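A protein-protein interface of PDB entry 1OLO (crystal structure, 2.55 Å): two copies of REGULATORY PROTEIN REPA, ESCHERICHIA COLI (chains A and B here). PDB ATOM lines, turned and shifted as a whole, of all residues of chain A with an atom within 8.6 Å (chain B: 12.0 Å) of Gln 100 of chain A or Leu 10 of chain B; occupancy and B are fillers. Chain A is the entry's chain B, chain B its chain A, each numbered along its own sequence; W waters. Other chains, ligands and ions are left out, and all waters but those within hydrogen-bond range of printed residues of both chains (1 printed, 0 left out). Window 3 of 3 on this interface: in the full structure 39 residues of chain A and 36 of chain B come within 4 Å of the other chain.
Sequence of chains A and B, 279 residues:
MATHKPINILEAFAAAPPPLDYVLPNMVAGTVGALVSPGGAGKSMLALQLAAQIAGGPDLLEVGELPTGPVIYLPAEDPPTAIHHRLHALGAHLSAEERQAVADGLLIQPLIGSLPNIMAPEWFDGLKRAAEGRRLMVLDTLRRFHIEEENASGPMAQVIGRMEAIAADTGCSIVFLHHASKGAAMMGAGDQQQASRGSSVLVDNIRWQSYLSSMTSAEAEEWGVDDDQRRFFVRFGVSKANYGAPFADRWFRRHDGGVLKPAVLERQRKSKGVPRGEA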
ATOM      1  N   ALA A  55     -33.697  -8.053   3.300  1.00  0.00           N
ATOM      2  CA  ALA A  55     -32.448  -8.227   2.553  1.00  0.00           C
ATOM      3  C   ALA A  55     -31.275  -8.473   3.481  1.00  0.00           C
ATOM      4  O   ALA A  55     -30.211  -8.885   3.032  1.00  0.00           O
ATOM      5  CB  ALA A  55     -32.163  -7.013   1.628  1.00  0.00           C
ATOM      6  N   GLY A  56     -31.457  -8.228   4.773  1.00  0.00           N
ATOM      7  CA  GLY A  56     -30.398  -8.475   5.750  1.00  0.00           C
ATOM      8  C   GLY A  56     -29.912  -7.262   6.528  1.00  0.00           C
ATOM      9  O   GLY A  56     -28.943  -7.380   7.275  1.00  0.00           O
ATOM     10  N   GLY A  57     -30.555  -6.101   6.367  1.00  0.00           N
ATOM     11  CA  GLY A  57     -30.288  -4.954   7.228  1.00  0.00           C
ATOM     12  C   GLY A  57     -31.001  -5.039   8.575  1.00  0.00           C
ATOM     13  O   GLY A  57     -31.779  -5.980   8.825  1.00  0.00           O
ATOM     14  N   LEU A  87     -32.203   6.413   0.313  1.00  0.00           N
ATOM     15  CA  LEU A  87     -31.144   5.474   0.605  1.00  0.00           C
ATOM     16  C   LEU A  87     -30.031   6.134   1.415  1.00  0.00           C
ATOM     17  O   LEU A  87     -29.603   5.598   2.442  1.00  0.00           O
ATOM     18  CB  LEU A  87     -30.575   4.867  -0.663  1.00  0.00           C
ATOM     19  CG  LEU A  87     -31.399   3.698  -1.137  1.00  0.00           C
ATOM     20  CD1 LEU A  87     -31.030   3.489  -2.575  1.00  0.00           C
ATOM     21  CD2 LEU A  87     -31.216   2.396  -0.314  1.00  0.00           C
ATOM     22  N   HIS A  88     -29.566   7.293   0.966  1.00  0.00           N
ATOM     23  CA  HIS A  88     -28.449   7.897   1.648  1.00  0.00           C
ATOM     24  C   HIS A  88     -28.861   8.161   3.094  1.00  0.00           C
ATOM     25  O   HIS A  88     -28.085   7.949   4.014  1.00  0.00           O
ATOM     26  CB  HIS A  88     -27.964   9.183   0.963  1.00  0.00           C
ATOM     27  CG  HIS A  88     -26.817   9.832   1.675  1.00  0.00           C
ATOM     28  ND1 HIS A  88     -25.565   9.245   1.768  1.00  0.00           N
ATOM     29  CD2 HIS A  88     -26.739  10.993   2.377  1.00  0.00           C
ATOM     30  CE1 HIS A  88     -24.763  10.030   2.472  1.00  0.00           C
ATOM     31  NE2 HIS A  88     -25.446  11.098   2.851  1.00  0.00           N
ATOM     32  N   GLY A  91     -28.872   5.086   5.033  1.00  0.00           N
ATOM     33  CA  GLY A  91     -27.513   4.612   5.156  1.00  0.00           C
ATOM     34  C   GLY A  91     -26.844   5.101   6.414  1.00  0.00           C
ATOM     35  O   GLY A  91     -26.063   4.337   7.022  1.00  0.00           O
ATOM     36  N   LEU A  94     -27.086   2.637   9.303  1.00  0.00           N
ATOM     37  CA  LEU A  94     -26.566   1.298   9.031  1.00  0.00           C
ATOM     38  C   LEU A  94     -25.019   1.276   9.232  1.00  0.00           C
ATOM     39  O   LEU A  94     -24.322   2.262   8.912  1.00  0.00           O
ATOM     40  CB  LEU A  94     -26.946   0.934   7.611  1.00  0.00           C
ATOM     41  CG  LEU A  94     -28.225   0.117   7.413  1.00  0.00           C
ATOM     42  CD1 LEU A  94     -29.450   0.741   8.048  1.00  0.00           C
ATOM     43  CD2 LEU A  94     -28.498  -0.167   5.925  1.00  0.00           C
ATOM     44  N   SER A  95     -24.506   0.181   9.807  1.00  0.00           N
ATOM     45  CA  SER A  95     -23.061  -0.080   9.900  1.00  0.00           C
ATOM     46  C   SER A  95     -22.530  -0.458   8.529  1.00  0.00           C
ATOM     47  O   SER A  95     -23.314  -0.848   7.618  1.00  0.00           O
ATOM     48  CB  SER A  95     -22.763  -1.245  10.848  1.00  0.00           C
ATOM     49  OG  SER A  95     -23.069  -2.472  10.210  1.00  0.00           O
ATOM     50  N   ALA A  96     -21.211  -0.400   8.381  1.00  0.00           N
ATOM     51  CA  ALA A  96     -20.598  -0.838   7.129  1.00  0.00           C
ATOM     52  C   ALA A  96     -21.098  -2.264   6.664  1.00  0.00           C
ATOM     53  O   ALA A  96     -21.388  -2.462   5.473  1.00  0.00           O
ATOM     54  CB  ALA A  96     -19.049  -0.708   7.203  1.00  0.00           C
ATOM     55  N   GLU A  97     -21.276  -3.206   7.594  1.00  0.00           N
ATOM     56  CA  GLU A  97     -21.683  -4.579   7.252  1.00  0.00           C
ATOM     57  C   GLU A  97     -23.136  -4.658   6.882  1.00  0.00           C
ATOM     58  O   GLU A  97     -23.535  -5.490   6.041  1.00  0.00           O
ATOM     59  CB  GLU A  97     -21.454  -5.563   8.412  1.00  0.00           C
ATOM     60  CG  GLU A  97     -19.991  -5.944   8.651  1.00  0.00           C
ATOM     61  CD  GLU A  97     -19.163  -4.932   9.489  1.00  0.00           C
ATOM     62  OE1 GLU A  97     -19.348  -3.665   9.468  1.00  0.00           O
ATOM     63  OE2 GLU A  97     -18.252  -5.430  10.188  1.00  0.00           O
ATOM     64  N   GLU A  98     -23.949  -3.838   7.550  1.00  0.00           N
ATOM     65  CA  GLU A  98     -25.386  -3.806   7.257  1.00  0.00           C
ATOM     66  C   GLU A  98     -25.623  -3.251   5.839  1.00  0.00           C
ATOM     67  O   GLU A  98     -26.379  -3.820   5.061  1.00  0.00           O
ATOM     68  CB  GLU A  98     -26.110  -2.967   8.308  1.00  0.00           C
ATOM     69  CG  GLU A  98     -26.456  -3.730   9.589  1.00  0.00           C
ATOM     70  CD  GLU A  98     -26.509  -2.818  10.817  1.00  0.00           C
ATOM     71  OE1 GLU A  98     -25.980  -1.680  10.786  1.00  0.00           O
ATOM     72  OE2 GLU A  98     -27.119  -3.235  11.818  1.00  0.00           O
ATOM     73  N   ARG A  99     -24.915  -2.172   5.521  1.00  0.00           N
ATOM     74  CA  ARG A  99     -24.941  -1.558   4.205  1.00  0.00           C
ATOM     75  C   ARG A  99     -24.613  -2.552   3.110  1.00  0.00           C
ATOM     76  O   ARG A  99     -25.314  -2.630   2.094  1.00  0.00           O
ATOM     77  CB  ARG A  99     -23.915  -0.468   4.142  1.00  0.00           C
ATOM     78  CG  ARG A  99     -24.268   0.772   4.890  1.00  0.00           C
ATOM     79  CD  ARG A  99     -23.180   1.808   4.744  1.00  0.00           C
ATOM     80  NE  ARG A  99     -23.281   2.764   5.831  1.00  0.00           N
ATOM     81  CZ  ARG A  99     -22.708   3.973   5.857  1.00  0.00           C
ATOM     82  NH1 ARG A  99     -21.952   4.412   4.851  1.00  0.00           N
ATOM     83  NH2 ARG A  99     -22.910   4.768   6.898  1.00  0.00           N
ATOM     84  N   GLN A 100     -23.545  -3.313   3.325  1.00  0.00           N
ATOM     85  CA  GLN A 100     -23.083  -4.297   2.367  1.00  0.00           C
ATOM     86  C   GLN A 100     -24.122  -5.399   2.199  1.00  0.00           C
ATOM     87  O   GLN A 100     -24.404  -5.844   1.065  1.00  0.00           O
ATOM     88  CB  GLN A 100     -21.724  -4.889   2.810  1.00  0.00           C
ATOM     89  CG  GLN A 100     -21.123  -5.873   1.786  1.00  0.00           C
ATOM     90  CD  GLN A 100     -20.761  -5.186   0.436  1.00  0.00           C
ATOM     91  OE1 GLN A 100     -19.875  -4.328   0.389  1.00  0.00           O
ATOM     92  NE2 GLN A 100     -21.464  -5.552  -0.638  1.00  0.00           N
ATOM     93  N   ALA A 101     -24.681  -5.870   3.317  1.00  0.00           N
ATOM     94  CA  ALA A 101     -25.733  -6.898   3.254  1.00  0.00           C
ATOM     95  C   ALA A 101     -26.934  -6.399   2.456  1.00  0.00           C
ATOM     96  O   ALA A 101     -27.469  -7.138   1.639  1.00  0.00           O
ATOM     97  CB  ALA A 101     -26.168  -7.337   4.642  1.00  0.00           C
ATOM     98  N   VAL A 102     -27.343  -5.146   2.688  1.00  0.00           N
ATOM     99  CA  VAL A 102     -28.451  -4.590   1.936  1.00  0.00           C
ATOM    100  C   VAL A 102     -28.087  -4.526   0.441  1.00  0.00           C
ATOM    101  O   VAL A 102     -28.862  -4.975  -0.416  1.00  0.00           O
ATOM    102  CB  VAL A 102     -28.919  -3.193   2.477  1.00  0.00           C
ATOM    103  CG1 VAL A 102     -29.891  -2.491   1.485  1.00  0.00           C
ATOM    104  CG2 VAL A 102     -29.532  -3.318   3.863  1.00  0.00           C
ATOM    105  N   ALA A 103     -26.936  -3.960   0.119  1.00  0.00           N
ATOM    106  CA  ALA A 103     -26.548  -3.905  -1.276  1.00  0.00           C
ATOM    107  C   ALA A 103     -26.482  -5.307  -1.900  1.00  0.00           C
ATOM    108  O   ALA A 103     -26.823  -5.444  -3.046  1.00  0.00           O
ATOM    109  CB  ALA A 103     -25.206  -3.147  -1.476  1.00  0.00           C
ATOM    110  N   ASP A 104     -26.033  -6.337  -1.172  1.00  0.00           N
ATOM    111  CA  ASP A 104     -26.028  -7.688  -1.750  1.00  0.00           C
ATOM    112  C   ASP A 104     -27.472  -8.179  -1.990  1.00  0.00           C
ATOM    113  O   ASP A 104     -27.793  -8.692  -3.097  1.00  0.00           O
ATOM    114  CB  ASP A 104     -25.324  -8.728  -0.850  1.00  0.00           C
ATOM    115  CG  ASP A 104     -23.824  -8.420  -0.589  1.00  0.00           C
ATOM    116  OD1 ASP A 104     -23.228  -7.584  -1.351  1.00  0.00           O
ATOM    117  OD2 ASP A 104     -23.183  -8.990   0.368  1.00  0.00           O
ATOM    118  N   GLY A 105     -28.318  -8.033  -0.956  1.00  0.00           N
ATOM    119  CA  GLY A 105     -29.660  -8.562  -0.972  1.00  0.00           C
ATOM    120  C   GLY A 105     -30.774  -7.817  -1.704  1.00  0.00           C
ATOM    121  O   GLY A 105     -31.789  -8.433  -1.997  1.00  0.00           O
ATOM    122  N   LEU A 106     -30.623  -6.515  -1.992  1.00  0.00           N
ATOM    123  CA  LEU A 106     -31.783  -5.715  -2.429  1.00  0.00           C
ATOM    124  C   LEU A 106     -31.599  -5.175  -3.822  1.00  0.00           C
ATOM    125  O   LEU A 106     -30.654  -4.454  -4.051  1.00  0.00           O
ATOM    126  CB  LEU A 106     -32.032  -4.554  -1.468  1.00  0.00           C
ATOM    127  CG  LEU A 106     -33.125  -3.510  -1.783  1.00  0.00           C
ATOM    128  CD1 LEU A 106     -34.530  -4.144  -2.004  1.00  0.00           C
ATOM    129  CD2 LEU A 106     -33.162  -2.429  -0.670  1.00  0.00           C
ATOM    130  N   LYS B   5     -31.371   2.124 -15.225  1.00  0.00           N
ATOM    131  CA  LYS B   5     -30.422   1.160 -14.707  1.00  0.00           C
ATOM    132  C   LYS B   5     -30.860   0.873 -13.236  1.00  0.00           C
ATOM    133  O   LYS B   5     -31.534   1.686 -12.635  1.00  0.00           O
ATOM    134  CB  LYS B   5     -28.955   1.644 -14.896  1.00  0.00           C
ATOM    135  CG  LYS B   5     -28.464   2.967 -14.200  1.00  0.00           C
ATOM    136  CD  LYS B   5     -27.220   2.714 -13.213  1.00  0.00           C
ATOM    137  CE  LYS B   5     -25.825   3.492 -13.501  1.00  0.00           C
ATOM    138  NZ  LYS B   5     -24.531   2.884 -12.840  1.00  0.00           N
ATOM    139  N   PRO B   6     -30.545  -0.274 -12.680  1.00  0.00           N
ATOM    140  CA  PRO B   6     -30.818  -0.514 -11.260  1.00  0.00           C
ATOM    141  C   PRO B   6     -30.146   0.513 -10.346  1.00  0.00           C
ATOM    142  O   PRO B   6     -29.100   1.029 -10.694  1.00  0.00           O
ATOM    143  CB  PRO B   6     -30.139  -1.857 -10.996  1.00  0.00           C
ATOM    144  CG  PRO B   6     -29.859  -2.445 -12.315  1.00  0.00           C
ATOM    145  CD  PRO B   6     -29.911  -1.423 -13.348  1.00  0.00           C
ATOM    146  N   ILE B   7     -30.695   0.805  -9.179  1.00  0.00           N
ATOM    147  CA  ILE B   7     -29.992   1.683  -8.274  1.00  0.00           C
ATOM    148  C   ILE B   7     -28.732   0.992  -7.777  1.00  0.00           C
ATOM    149  O   ILE B   7     -28.758  -0.152  -7.361  1.00  0.00           O
ATOM    150  CB  ILE B   7     -30.879   2.124  -7.082  1.00  0.00           C
ATOM    151  CG1 ILE B   7     -32.196   2.777  -7.541  1.00  0.00           C
ATOM    152  CG2 ILE B   7     -30.077   2.996  -6.083  1.00  0.00           C
ATOM    153  CD1 ILE B   7     -32.064   3.942  -8.337  1.00  0.00           C
ATOM    154  N   ASN B   8     -27.626   1.720  -7.821  1.00  0.00           N
ATOM    155  CA  ASN B   8     -26.415   1.277  -7.201  1.00  0.00           C
ATOM    156  C   ASN B   8     -26.462   1.650  -5.724  1.00  0.00           C
ATOM    157  O   ASN B   8     -26.211   2.800  -5.371  1.00  0.00           O
ATOM    158  CB  ASN B   8     -25.242   1.980  -7.854  1.00  0.00           C
ATOM    159  CG  ASN B   8     -23.885   1.475  -7.363  1.00  0.00           C
ATOM    160  OD1 ASN B   8     -23.715   0.821  -6.314  1.00  0.00           O
ATOM    161  ND2 ASN B   8     -22.896   1.799  -8.145  1.00  0.00           N
ATOM    162  N   ILE B   9     -26.757   0.682  -4.874  1.00  0.00           N
ATOM    163  CA  ILE B   9     -26.997   0.950  -3.478  1.00  0.00           C
ATOM    164  C   ILE B   9     -25.755   1.345  -2.667  1.00  0.00           C
ATOM    165  O   ILE B   9     -25.822   2.308  -1.920  1.00  0.00           O
ATOM    166  CB  ILE B   9     -27.754  -0.250  -2.870  1.00  0.00           C
ATOM    167  CG1 ILE B   9     -29.161  -0.329  -3.491  1.00  0.00           C
ATOM    168  CG2 ILE B   9     -27.753  -0.242  -1.332  1.00  0.00           C
ATOM    169  CD1 ILE B   9     -29.791  -1.589  -3.164  1.00  0.00           C
ATOM    170  N   LEU B  10     -24.631   0.634  -2.800  1.00  0.00           N
ATOM    171  CA  LEU B  10     -23.395   0.997  -2.089  1.00  0.00           C
ATOM    172  C   LEU B  10     -23.048   2.431  -2.404  1.00  0.00           C
ATOM    173  O   LEU B  10     -22.700   3.208  -1.531  1.00  0.00           O
ATOM    174  CB  LEU B  10     -22.227   0.138  -2.513  1.00  0.00           C
ATOM    175  CG  LEU B  10     -22.225  -1.171  -1.780  1.00  0.00           C
ATOM    176  CD1 LEU B  10     -21.240  -2.088  -2.445  1.00  0.00           C
ATOM    177  CD2 LEU B  10     -21.894  -0.997  -0.310  1.00  0.00           C
ATOM    178  N   GLU B  11     -23.160   2.786  -3.667  1.00  0.00           N
ATOM    179  CA  GLU B  11     -22.763   4.077  -4.056  1.00  0.00           C
ATOM    180  C   GLU B  11     -23.683   5.151  -3.383  1.00  0.00           C
ATOM    181  O   GLU B  11     -23.187   6.175  -2.880  1.00  0.00           O
ATOM    182  CB  GLU B  11     -22.732   4.116  -5.581  1.00  0.00           C
ATOM    183  CG  GLU B  11     -22.245   5.428  -6.204  1.00  0.00           C
ATOM    184  CD  GLU B  11     -22.822   5.649  -7.594  1.00  0.00           C
ATOM    185  OE1 GLU B  11     -22.502   4.842  -8.513  1.00  0.00           O
ATOM    186  OE2 GLU B  11     -23.610   6.603  -7.770  1.00  0.00           O
ATOM    187  N   ALA B  12     -24.996   4.910  -3.334  1.00  0.00           N
ATOM    188  CA  ALA B  12     -25.924   5.828  -2.675  1.00  0.00           C
ATOM    189  C   ALA B  12     -25.704   5.946  -1.157  1.00  0.00           C
ATOM    190  O   ALA B  12     -25.884   7.018  -0.606  1.00  0.00           O
ATOM    191  CB  ALA B  12     -27.348   5.461  -2.998  1.00  0.00           C
ATOM    192  N   PHE B  13     -25.300   4.870  -0.492  1.00  0.00           N
ATOM    193  CA  PHE B  13     -24.957   4.929   0.917  1.00  0.00           C
ATOM    194  C   PHE B  13     -23.627   5.669   1.200  1.00  0.00           C
ATOM    195  O   PHE B  13     -23.436   6.260   2.278  1.00  0.00           O
ATOM    196  CB  PHE B  13     -24.724   3.523   1.469  1.00  0.00           C
ATOM    197  CG  PHE B  13     -25.953   2.706   1.680  1.00  0.00           C
ATOM    198  CD1 PHE B  13     -27.195   3.288   1.835  1.00  0.00           C
ATOM    199  CD2 PHE B  13     -25.847   1.319   1.733  1.00  0.00           C
ATOM    200  CE1 PHE B  13     -28.303   2.502   2.046  1.00  0.00           C
ATOM    201  CE2 PHE B  13     -26.946   0.526   1.957  1.00  0.00           C
ATOM    202  CZ  PHE B  13     -28.176   1.113   2.116  1.00  0.00           C
ATOM    203  N   ALA B  14     -22.663   5.538   0.286  1.00  0.00           N
ATOM    204  CA  ALA B  14     -21.248   5.801   0.619  1.00  0.00           C
ATOM    205  C   ALA B  14     -20.947   7.266   0.404  1.00  0.00           C
ATOM    206  O   ALA B  14     -20.006   7.790   1.012  1.00  0.00           O
ATOM    207  CB  ALA B  14     -20.288   4.915  -0.202  1.00  0.00           C
ATOM    208  N   ALA B  15     -21.756   7.919  -0.442  1.00  0.00           N
ATOM    209  CA  ALA B  15     -21.630   9.350  -0.663  1.00  0.00           C
ATOM    210  C   ALA B  15     -22.971  10.094  -0.819  1.00  0.00           C
ATOM    211  O   ALA B  15     -23.889   9.630  -1.519  1.00  0.00           O
ATOM    212  CB  ALA B  15     -20.761   9.606  -1.874  1.00  0.00           C
ATOM    213  N   ALA B  16     -23.047  11.257  -0.158  1.00  0.00           N
ATOM    214  CA  ALA B  16     -24.074  12.296  -0.355  1.00  0.00           C
ATOM    215  C   ALA B  16     -24.407  12.521  -1.813  1.00  0.00           C
ATOM    216  O   ALA B  16     -23.589  13.038  -2.575  1.00  0.00           O
ATOM    217  CB  ALA B  16     -23.625  13.650   0.278  1.00  0.00           C
ATOM    218  N   PRO B  17     -25.619  12.156  -2.207  1.00  0.00           N
ATOM    219  CA  PRO B  17     -26.064  12.461  -3.562  1.00  0.00           C
ATOM    220  C   PRO B  17     -26.008  13.982  -3.754  1.00  0.00           C
ATOM    221  O   PRO B  17     -26.104  14.727  -2.767  1.00  0.00           O
ATOM    222  CB  PRO B  17     -27.527  11.953  -3.578  1.00  0.00           C
ATOM    223  CG  PRO B  17     -27.599  10.946  -2.515  1.00  0.00           C
ATOM    224  CD  PRO B  17     -26.667  11.475  -1.420  1.00  0.00           C
ATOM    225  N   PRO B  18     -25.860  14.444  -4.990  1.00  0.00           N
ATOM    226  CA  PRO B  18     -26.073  15.875  -5.262  1.00  0.00           C
ATOM    227  C   PRO B  18     -27.480  16.234  -4.734  1.00  0.00           C
ATOM    228  O   PRO B  18     -28.355  15.369  -4.714  1.00  0.00           O
ATOM    229  CB  PRO B  18     -26.054  15.963  -6.803  1.00  0.00           C
ATOM    230  CG  PRO B  18     -26.067  14.507  -7.315  1.00  0.00           C
ATOM    231  CD  PRO B  18     -25.529  13.655  -6.198  1.00  0.00           C
HETATM  232  O   HOH W   1     -25.649   6.752   4.154  1.00  0.00           O
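Leu 87 of chain A touches Ile 7 of chain B (CD1 to CG2, 3.7 Å).
Phe 13 of chain B touches Leu 87 of chain A.
Phe 13 of chain B touches His 88 of chain A (O to ND1, 3.7 Å).
N of Ala 16 of chain B touches CE1 of His 88 of chain A (3.4 Å).
CG of His 88 of chain A touches CD of Pro 17 of chain B (3.5 Å).
Gly 91 of chain A touches Phe 13 of chain B (CA to CD1, 3.6 Å).
Leu 10 of chain B touches Gln 100 of chain A.
Ile 9 of chain B touches Ala 103 of chain A (CG2 to CA, 3.9 Å).
Leu 10 of chain B touches Ala 103 of chain A (CG to CB, 3.6 Å).
Leu 106 of chain A touches Ile 9 of chain B.
Hydrophobic or aromatic side chains of chain B within 4 Å of the printed part of chain A: Ile 7, Ile 9, Leu 10, Phe 13 and Pro 17.
Along chain B the printed residues that touch a printed residue of chain A span positions 7 to 17.
Of the 19 printed residues of chain A, 7 touch a printed residue of chain B.
Hydrophobic or aromatic side chains of chain A within 4 Å of the printed part of chain B: Leu 87, His 88 and Ala 103.
Along chain A the printed residues that touch a printed residue of chain B span positions 87 to 106.
Among the printed residues, 13 pairs touch across the chains.
A ring nitrogen (ND1) of His 88 of chain A lies within hydrogen-bond range of the backbone carbonyl oxygen (O) of Ala 12 of chain B (3.3 Å).
The guanidinium group (NH1) of Arg 99 of chain A lies within hydrogen-bond range of the backbone carbonyl oxygen (O) of Phe 13 of chain B (3.5 Å).
Gln 100 of chain A touches just one residue of chain B: Leu 10 (3.9 Å).
Leu 10 of chain B touches just these residues of chain A: Gln 100 and Ala 103.
Ala 96 of chain A touches none of the printed residues of chain B.
No residue of chain B comes within 4 Å of Ala 101 of chain A.
No residue of chain B comes within 4 Å of Val 102 of chain A.
Printed residues of chain B within 4 Å of Ala 103 of chain A: Ile 9 (3.9 Å) and Leu 10 (3.6 Å).
Of the printed residues of chain A, Ile 9 of chain B touches Ala 103 and Leu 106.
Printed residues of chain A within 4 Å of Pro 17 of chain B: His 88.
Glu 97 of chain A touches none of the printed residues of chain B.
The nearest residue of chain B that does not touch Gln 100 of chain A is Phe 13 of chain B (5.3 Å).
No position is printed for both chains.
Of the 13 pairs that touch across the chains among the printed residues, none has its exchanged pair printed and touching as well.
Water W1 lies within hydrogen-bond range of the backbone carbonyl oxygen of His 88 of chain A and the backbone carbonyl oxygen of Phe 13 of chain B.
The backbone carbonyl oxygen of Gly 91 of chain A sits at hydrogen-bond distance from the guanidinium group of Arg 99 of chain A.
The backbone carbonyl oxygen of Leu 94 of chain A lies within hydrogen-bond range of the guanidinium group of Arg 99 of chain A (3.3 Å).
The side-chain amide nitrogen (NE2) of Gln 100 of chain A lies within hydrogen-bond range of the side-chain carboxylate (OD1) of Asp 104 of chain A, at 2.8 Å.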
